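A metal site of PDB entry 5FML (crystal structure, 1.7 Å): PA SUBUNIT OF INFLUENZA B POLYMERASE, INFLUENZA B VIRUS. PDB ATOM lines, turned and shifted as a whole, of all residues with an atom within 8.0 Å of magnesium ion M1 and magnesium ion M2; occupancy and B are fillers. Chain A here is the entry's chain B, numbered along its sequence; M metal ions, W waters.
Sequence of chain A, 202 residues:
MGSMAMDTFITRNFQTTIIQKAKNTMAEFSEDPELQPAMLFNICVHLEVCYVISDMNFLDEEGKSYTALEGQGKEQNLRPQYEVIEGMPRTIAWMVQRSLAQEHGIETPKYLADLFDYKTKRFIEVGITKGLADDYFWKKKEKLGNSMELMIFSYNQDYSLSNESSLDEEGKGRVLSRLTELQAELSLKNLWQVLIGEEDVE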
ATOM      1  N   THR A  25       0.121  22.358  -1.688  1.00  0.00           N
ATOM      2  CA  THR A  25       0.953  22.845  -0.571  1.00  0.00           C
ATOM      3  C   THR A  25       2.270  23.404  -1.066  1.00  0.00           C
ATOM      4  O   THR A  25       2.662  24.494  -0.695  1.00  0.00           O
ATOM      5  CB  THR A  25       1.212  21.739   0.458  1.00  0.00           C
ATOM      6  OG1 THR A  25      -0.053  21.260   0.923  1.00  0.00           O
ATOM      7  CG2 THR A  25       2.096  22.208   1.619  1.00  0.00           C
ATOM      8  N   PHE A  29       3.665  27.182  -0.917  1.00  0.00           N
ATOM      9  CA  PHE A  29       5.040  27.491  -0.477  1.00  0.00           C
ATOM     10  C   PHE A  29       5.984  27.905  -1.610  1.00  0.00           C
ATOM     11  O   PHE A  29       7.191  28.024  -1.367  1.00  0.00           O
ATOM     12  CB  PHE A  29       5.640  26.289   0.300  1.00  0.00           C
ATOM     13  CG  PHE A  29       4.914  25.931   1.604  1.00  0.00           C
ATOM     14  CD1 PHE A  29       4.393  26.918   2.455  1.00  0.00           C
ATOM     15  CD2 PHE A  29       4.797  24.598   2.005  1.00  0.00           C
ATOM     16  CE1 PHE A  29       3.764  26.571   3.655  1.00  0.00           C
ATOM     17  CE2 PHE A  29       4.174  24.258   3.201  1.00  0.00           C
ATOM     18  CZ  PHE A  29       3.642  25.239   4.019  1.00  0.00           C
ATOM     19  N   HIS A  46       2.686  13.035   5.330  1.00  0.00           N
ATOM     20  CA  HIS A  46       2.095  13.856   6.388  1.00  0.00           C
ATOM     21  C   HIS A  46       0.597  13.989   6.263  1.00  0.00           C
ATOM     22  O   HIS A  46      -0.157  13.802   7.231  1.00  0.00           O
ATOM     23  CB  HIS A  46       2.735  15.217   6.380  1.00  0.00           C
ATOM     24  CG  HIS A  46       2.426  16.020   7.586  1.00  0.00           C
ATOM     25  ND1 HIS A  46       1.402  16.944   7.621  1.00  0.00           N
ATOM     26  CD2 HIS A  46       3.015  16.059   8.792  1.00  0.00           C
ATOM     27  CE1 HIS A  46       1.358  17.491   8.817  1.00  0.00           C
ATOM     28  NE2 HIS A  46       2.346  17.003   9.534  1.00  0.00           N
ATOM     29  N   LEU A  47       0.153  14.305   5.053  1.00  0.00           N
ATOM     30  CA  LEU A  47      -1.265  14.351   4.773  1.00  0.00           C
ATOM     31  C   LEU A  47      -1.976  13.041   5.087  1.00  0.00           C
ATOM     32  O   LEU A  47      -3.013  13.017   5.790  1.00  0.00           O
ATOM     33  CB  LEU A  47      -1.455  14.695   3.285  1.00  0.00           C
ATOM     34  CG  LEU A  47      -1.204  16.142   2.855  1.00  0.00           C
ATOM     35  CD1 LEU A  47      -0.862  16.188   1.387  1.00  0.00           C
ATOM     36  CD2 LEU A  47      -2.410  17.044   3.143  1.00  0.00           C
ATOM     37  N   CYS A  50      -2.368  12.400   8.883  1.00  0.00           N
ATOM     38  CA  CYS A  50      -3.422  13.203   9.478  1.00  0.00           C
ATOM     39  C   CYS A  50      -4.812  12.665   9.204  1.00  0.00           C
ATOM     40  O   CYS A  50      -5.640  12.552  10.107  1.00  0.00           O
ATOM     41  CB  CYS A  50      -3.296  14.654   9.070  1.00  0.00           C
ATOM     42  SG  CYS A  50      -1.768  15.479   9.680  1.00  0.00           S
ATOM     43  N   ILE A  85      -7.173  19.769   9.915  1.00  0.00           N
ATOM     44  CA  ILE A  85      -6.860  21.114   9.456  1.00  0.00           C
ATOM     45  C   ILE A  85      -5.872  21.019   8.319  1.00  0.00           C
ATOM     46  O   ILE A  85      -6.010  21.687   7.315  1.00  0.00           O
ATOM     47  CB  ILE A  85      -6.343  21.980  10.620  1.00  0.00           C
ATOM     48  CG1 ILE A  85      -7.472  22.182  11.625  1.00  0.00           C
ATOM     49  CG2 ILE A  85      -5.827  23.333  10.111  1.00  0.00           C
ATOM     50  CD1 ILE A  85      -7.072  22.766  12.969  1.00  0.00           C
ATOM     51  N   GLU A  86      -4.862  20.155   8.454  1.00  0.00           N
ATOM     52  CA  GLU A  86      -3.957  19.845   7.369  1.00  0.00           C
ATOM     53  C   GLU A  86      -4.744  19.326   6.144  1.00  0.00           C
ATOM     54  O   GLU A  86      -5.665  18.520   6.253  1.00  0.00           O
ATOM     55  CB  GLU A  86      -2.925  18.824   7.822  1.00  0.00           C
ATOM     56  CG  GLU A  86      -1.925  18.439   6.739  1.00  0.00           C
ATOM     57  CD  GLU A  86      -1.098  19.612   6.266  1.00  0.00           C
ATOM     58  OE1 GLU A  86      -0.147  20.033   6.957  1.00  0.00           O
ATOM     59  OE2 GLU A  86      -1.433  20.192   5.216  1.00  0.00           O
ATOM     60  N   GLY A  87      -4.359  19.809   4.972  1.00  0.00           N
ATOM     61  CA  GLY A  87      -4.959  19.380   3.719  1.00  0.00           C
ATOM     62  C   GLY A  87      -6.021  20.336   3.207  1.00  0.00           C
ATOM     63  O   GLY A  87      -6.342  20.260   2.045  1.00  0.00           O
ATOM     64  N   ARG A  90      -4.481  26.601   2.789  1.00  0.00           N
ATOM     65  CA  ARG A  90      -3.943  27.179   4.028  1.00  0.00           C
ATOM     66  C   ARG A  90      -4.658  28.406   4.506  1.00  0.00           C
ATOM     67  O   ARG A  90      -4.866  28.592   5.695  1.00  0.00           O
ATOM     68  CB  ARG A  90      -2.417  27.411   3.967  1.00  0.00           C
ATOM     69  CG  ARG A  90      -1.599  26.160   4.269  1.00  0.00           C
ATOM     70  CD  ARG A  90      -0.104  26.423   4.203  1.00  0.00           C
ATOM     71  NE  ARG A  90       0.380  27.234   5.328  1.00  0.00           N
ATOM     72  CZ  ARG A  90       0.904  26.774   6.467  1.00  0.00           C
ATOM     73  NH1 ARG A  90       1.034  25.468   6.710  1.00  0.00           N
ATOM     74  NH2 ARG A  90       1.315  27.648   7.398  1.00  0.00           N
ATOM     75  N   LEU A 112       0.036  27.146  12.528  1.00  0.00           N
ATOM     76  CA  LEU A 112      -1.087  26.410  12.003  1.00  0.00           C
ATOM     77  C   LEU A 112      -0.956  24.927  12.410  1.00  0.00           C
ATOM     78  O   LEU A 112       0.057  24.290  12.150  1.00  0.00           O
ATOM     79  CB  LEU A 112      -1.143  26.526  10.483  1.00  0.00           C
ATOM     80  CG  LEU A 112      -2.427  26.009   9.818  1.00  0.00           C
ATOM     81  CD1 LEU A 112      -3.698  26.708  10.256  1.00  0.00           C
ATOM     82  CD2 LEU A 112      -2.291  26.085   8.301  1.00  0.00           C
ATOM     83  N   ALA A 113      -1.983  24.444  13.084  1.00  0.00           N
ATOM     84  CA  ALA A 113      -2.005  23.071  13.581  1.00  0.00           C
ATOM     85  C   ALA A 113      -2.361  22.131  12.441  1.00  0.00           C
ATOM     86  O   ALA A 113      -2.792  22.548  11.384  1.00  0.00           O
ATOM     87  CB  ALA A 113      -3.012  22.936  14.677  1.00  0.00           C
ATOM     88  N   ASP A 114      -2.179  20.868  12.687  1.00  0.00           N
ATOM     89  CA  ASP A 114      -2.653  19.807  11.783  1.00  0.00           C
ATOM     90  C   ASP A 114      -4.033  19.211  12.104  1.00  0.00           C
ATOM     91  O   ASP A 114      -4.786  18.890  11.165  1.00  0.00           O
ATOM     92  CB  ASP A 114      -1.672  18.690  11.795  1.00  0.00           C
ATOM     93  CG  ASP A 114      -0.375  19.089  11.208  1.00  0.00           C
ATOM     94  OD1 ASP A 114      -0.385  19.841  10.215  1.00  0.00           O
ATOM     95  OD2 ASP A 114       0.641  18.611  11.704  1.00  0.00           O
ATOM     96  N   LEU A 115      -4.355  19.074  13.403  1.00  0.00           N
ATOM     97  CA  LEU A 115      -5.617  18.561  13.885  1.00  0.00           C
ATOM     98  C   LEU A 115      -6.089  19.356  15.047  1.00  0.00           C
ATOM     99  O   LEU A 115      -5.282  20.045  15.692  1.00  0.00           O
ATOM    100  CB  LEU A 115      -5.550  17.071  14.294  1.00  0.00           C
ATOM    101  CG  LEU A 115      -4.807  16.074  13.440  1.00  0.00           C
ATOM    102  CD1 LEU A 115      -4.513  14.850  14.321  1.00  0.00           C
ATOM    103  CD2 LEU A 115      -5.712  15.693  12.308  1.00  0.00           C
ATOM    104  N   ILE A 124      -3.253  19.860  17.673  1.00  0.00           N
ATOM    105  CA  ILE A 124      -2.273  18.843  17.515  1.00  0.00           C
ATOM    106  C   ILE A 124      -1.367  19.166  16.339  1.00  0.00           C
ATOM    107  O   ILE A 124      -1.811  19.562  15.276  1.00  0.00           O
ATOM    108  CB  ILE A 124      -2.944  17.489  17.287  1.00  0.00           C
ATOM    109  CG1 ILE A 124      -3.774  17.095  18.541  1.00  0.00           C
ATOM    110  CG2 ILE A 124      -1.930  16.439  16.934  1.00  0.00           C
ATOM    111  CD1 ILE A 124      -4.758  15.983  18.266  1.00  0.00           C
ATOM    112  N   GLU A 125      -0.075  18.969  16.531  1.00  0.00           N
ATOM    113  CA  GLU A 125       0.888  19.009  15.439  1.00  0.00           C
ATOM    114  C   GLU A 125       1.428  17.591  15.247  1.00  0.00           C
ATOM    115  O   GLU A 125       1.874  16.900  16.204  1.00  0.00           O
ATOM    116  CB  GLU A 125       2.015  19.986  15.810  1.00  0.00           C
ATOM    117  CG  GLU A 125       3.238  19.877  14.952  1.00  0.00           C
ATOM    118  CD  GLU A 125       3.119  20.587  13.658  1.00  0.00           C
ATOM    119  OE1 GLU A 125       2.086  21.283  13.376  1.00  0.00           O
ATOM    120  OE2 GLU A 125       4.093  20.467  12.895  1.00  0.00           O
ATOM    121  N   VAL A 126       1.327  17.091  14.019  1.00  0.00           N
ATOM    122  CA  VAL A 126       1.824  15.789  13.687  1.00  0.00           C
ATOM    123  C   VAL A 126       3.176  15.926  13.007  1.00  0.00           C
ATOM    124  O   VAL A 126       3.353  16.781  12.116  1.00  0.00           O
ATOM    125  CB  VAL A 126       0.756  15.008  12.775  1.00  0.00           C
ATOM    126  CG1 VAL A 126       1.343  13.746  12.212  1.00  0.00           C
ATOM    127  CG2 VAL A 126      -0.506  14.707  13.551  1.00  0.00           C
ATOM    128  N   GLY A 127       4.140  15.126  13.456  1.00  0.00           N
ATOM    129  CA  GLY A 127       5.459  15.022  12.844  1.00  0.00           C
ATOM    130  C   GLY A 127       5.832  13.613  12.448  1.00  0.00           C
ATOM    131  O   GLY A 127       5.490  12.638  13.128  1.00  0.00           O
ATOM    132  N   ILE A 128       6.516  13.489  11.299  1.00  0.00           N
ATOM    133  CA  ILE A 128       6.978  12.217  10.754  1.00  0.00           C
ATOM    134  C   ILE A 128       8.485  12.309  10.492  1.00  0.00           C
ATOM    135  O   ILE A 128       8.940  13.206   9.768  1.00  0.00           O
ATOM    136  CB  ILE A 128       6.338  11.912   9.388  1.00  0.00           C
ATOM    137  CG1 ILE A 128       4.801  12.084   9.465  1.00  0.00           C
ATOM    138  CG2 ILE A 128       6.766  10.518   8.929  1.00  0.00           C
ATOM    139  CD1 ILE A 128       4.109  11.002  10.214  1.00  0.00           C
ATOM    140  N   TYR A 136      12.984  14.713  17.590  1.00  0.00           N
ATOM    141  CA  TYR A 136      12.115  15.619  16.853  1.00  0.00           C
ATOM    142  C   TYR A 136      11.071  16.271  17.766  1.00  0.00           C
ATOM    143  O   TYR A 136      10.806  17.457  17.635  1.00  0.00           O
ATOM    144  CB  TYR A 136      11.472  14.849  15.721  1.00  0.00           C
ATOM    145  CG  TYR A 136      10.642  15.661  14.740  1.00  0.00           C
ATOM    146  CD1 TYR A 136       9.296  15.879  14.942  1.00  0.00           C
ATOM    147  CD2 TYR A 136      11.217  16.206  13.600  1.00  0.00           C
ATOM    148  CE1 TYR A 136       8.531  16.604  14.045  1.00  0.00           C
ATOM    149  CE2 TYR A 136      10.460  16.915  12.677  1.00  0.00           C
ATOM    150  CZ  TYR A 136       9.135  17.114  12.897  1.00  0.00           C
ATOM    151  OH  TYR A 136       8.397  17.828  11.985  1.00  0.00           O
ATOM    152  N   LYS A 140      10.607  20.326  18.031  1.00  0.00           N
ATOM    153  CA  LYS A 140       9.324  21.020  17.803  1.00  0.00           C
ATOM    154  C   LYS A 140       8.777  21.717  19.040  1.00  0.00           C
ATOM    155  O   LYS A 140       8.137  22.753  18.919  1.00  0.00           O
ATOM    156  CB  LYS A 140       8.278  20.067  17.206  1.00  0.00           C
ATOM    157  CG  LYS A 140       8.559  19.760  15.761  1.00  0.00           C
ATOM    158  CD  LYS A 140       8.075  20.880  14.838  1.00  0.00           C
ATOM    159  CE  LYS A 140       8.583  20.717  13.411  1.00  0.00           C
ATOM    160  NZ  LYS A 140       8.901  22.026  12.769  1.00  0.00           N
ATOM    161  N   LEU A 144       6.950  25.378  19.661  1.00  0.00           N
ATOM    162  CA  LEU A 144       5.547  25.273  20.003  1.00  0.00           C
ATOM    163  C   LEU A 144       5.238  25.448  21.483  1.00  0.00           C
ATOM    164  O   LEU A 144       4.137  25.889  21.805  1.00  0.00           O
ATOM    165  CB  LEU A 144       4.984  23.932  19.535  1.00  0.00           C
ATOM    166  CG  LEU A 144       4.889  23.804  18.003  1.00  0.00           C
ATOM    167  CD1 LEU A 144       4.591  22.363  17.634  1.00  0.00           C
ATOM    168  CD2 LEU A 144       3.850  24.751  17.439  1.00  0.00           C
ATOM    169  N   MET A 148       0.478  23.186  21.536  1.00  0.00           N
ATOM    170  CA  MET A 148      -0.119  22.024  20.878  1.00  0.00           C
ATOM    171  C   MET A 148       0.364  20.711  21.457  1.00  0.00           C
ATOM    172  O   MET A 148       1.482  20.590  21.975  1.00  0.00           O
ATOM    173  CB  MET A 148       0.210  21.981  19.386  1.00  0.00           C
ATOM    174  CG  MET A 148      -0.160  23.231  18.640  1.00  0.00           C
ATOM    175  SD  MET A 148       0.137  22.984  16.886  1.00  0.00           S
ATOM    176  CE  MET A 148      -0.315  24.611  16.358  1.00  0.00           C
ATOM    177  N   LEU A 150       1.946  17.378  20.577  1.00  0.00           N
ATOM    178  CA  LEU A 150       2.761  16.786  19.520  1.00  0.00           C
ATOM    179  C   LEU A 150       2.538  15.317  19.410  1.00  0.00           C
ATOM    180  O   LEU A 150       2.582  14.598  20.449  1.00  0.00           O
ATOM    181  CB  LEU A 150       4.246  17.051  19.774  1.00  0.00           C
ATOM    182  CG  LEU A 150       4.683  18.504  19.520  1.00  0.00           C
ATOM    183  CD1 LEU A 150       6.006  18.785  20.227  1.00  0.00           C
ATOM    184  CD2 LEU A 150       4.886  18.738  18.036  1.00  0.00           C
ATOM    185  N   MET A 151       2.290  14.850  18.176  1.00  0.00           N
ATOM    186  CA  MET A 151       2.212  13.439  17.845  1.00  0.00           C
ATOM    187  C   MET A 151       3.281  13.101  16.807  1.00  0.00           C
ATOM    188  O   MET A 151       3.188  13.521  15.625  1.00  0.00           O
ATOM    189  CB  MET A 151       0.824  13.095  17.253  1.00  0.00           C
ATOM    190  CG  MET A 151      -0.338  13.098  18.209  1.00  0.00           C
ATOM    191  SD  MET A 151      -1.873  12.676  17.287  1.00  0.00           S
ATOM    192  CE  MET A 151      -3.096  12.377  18.533  1.00  0.00           C
ATOM    193  N   ILE A 152       4.299  12.356  17.232  1.00  0.00           N
ATOM    194  CA  ILE A 152       5.460  12.078  16.417  1.00  0.00           C
ATOM    195  C   ILE A 152       5.564  10.612  16.094  1.00  0.00           C
ATOM    196  O   ILE A 152       5.464   9.733  16.990  1.00  0.00           O
ATOM    197  CB  ILE A 152       6.802  12.553  17.072  1.00  0.00           C
ATOM    198  CG1 ILE A 152       6.707  13.953  17.636  1.00  0.00           C
ATOM    199  CG2 ILE A 152       7.963  12.416  16.097  1.00  0.00           C
ATOM    200  CD1 ILE A 152       6.306  15.053  16.672  1.00  0.00           C
ATOM    201  N   GLU A 198      11.354  15.081   7.327  1.00  0.00           N
ATOM    202  CA  GLU A 198      10.846  16.340   7.925  1.00  0.00           C
ATOM    203  C   GLU A 198      11.814  16.988   8.941  1.00  0.00           C
ATOM    204  O   GLU A 198      11.812  18.209   9.130  1.00  0.00           O
ATOM    205  CB  GLU A 198       9.489  16.144   8.608  1.00  0.00           C
ATOM    206  CG  GLU A 198       8.372  15.602   7.707  1.00  0.00           C
ATOM    207  CD  GLU A 198       6.997  15.622   8.365  1.00  0.00           C
ATOM    208  OE1 GLU A 198       6.863  15.864   9.595  1.00  0.00           O
ATOM    209  OE2 GLU A 198       6.024  15.373   7.626  1.00  0.00           O
HETATM  210 MG    MG M   1       2.441  18.482  11.373  1.00  0.00          MG
HETATM  211 MG    MG M   2       1.169  20.924   9.193  1.00  0.00          MG
HETATM  212  O   HOH W   1      -1.529  22.261   8.866  1.00  0.00           O
HETATM  213  O   HOH W   2       2.588  20.249  10.506  1.00  0.00           O
HETATM  214  O   HOH W   3       0.767  22.243  11.128  1.00  0.00           O
HETATM  215  O   HOH W   4       2.329  22.724   8.634  1.00  0.00           O
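Water W1 lies within hydrogen-bond range of O of Ala 113 (2.8 Å) and OE1 of Glu 86 (3.2 Å).
Residues that only touch magnesium ion M1: Glu 125 (3.0 Å).
Of the 26 residues printed, 4 come within 4 Å of magnesium ion M1.
Along chain A the residues within 4 Å of magnesium ion M1 span positions 46 to 126.
Magnesium ion M2 is bound by water W2 (2.0 Å), the side-chain carboxylate (OD1) of Asp 114 (2.2 Å), water W4 (2.2 Å) and water W3 (2.4 Å).
Magnesium ion M2 has four donor atoms within binding distance.
Slightly farther from magnesium ion M2 lies OE1 of Glu 86 (2.7 Å).
The backbone NH (N) of Asp 114 lies within hydrogen-bond range of the backbone carbonyl oxygen (O) of Ile 124.
N of Met 151 lies within hydrogen-bond range of O of Glu 125 (2.9 Å).
The backbone carbonyl oxygen (O) of Asp 114 lies within hydrogen-bond range of the backbone NH (N) of Glu 86.
O of Asp 114 lies within hydrogen-bond range of N of Ile 85, 2.8 Å away.
SG of Cys 50 sits at hydrogen-bond distance from O of His 46 (3.4 Å).
Magnesium ion M1 is bound by OD2 of Asp 114, water W2, O of Val 126 and NE2 of His 46.
Three residues have an atom within 4 Å of magnesium ion M2: His 46, Glu 86 and Asp 114.
The nearest printed residue that does not touch magnesium ion M2 is Glu 125 (4.3 Å).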
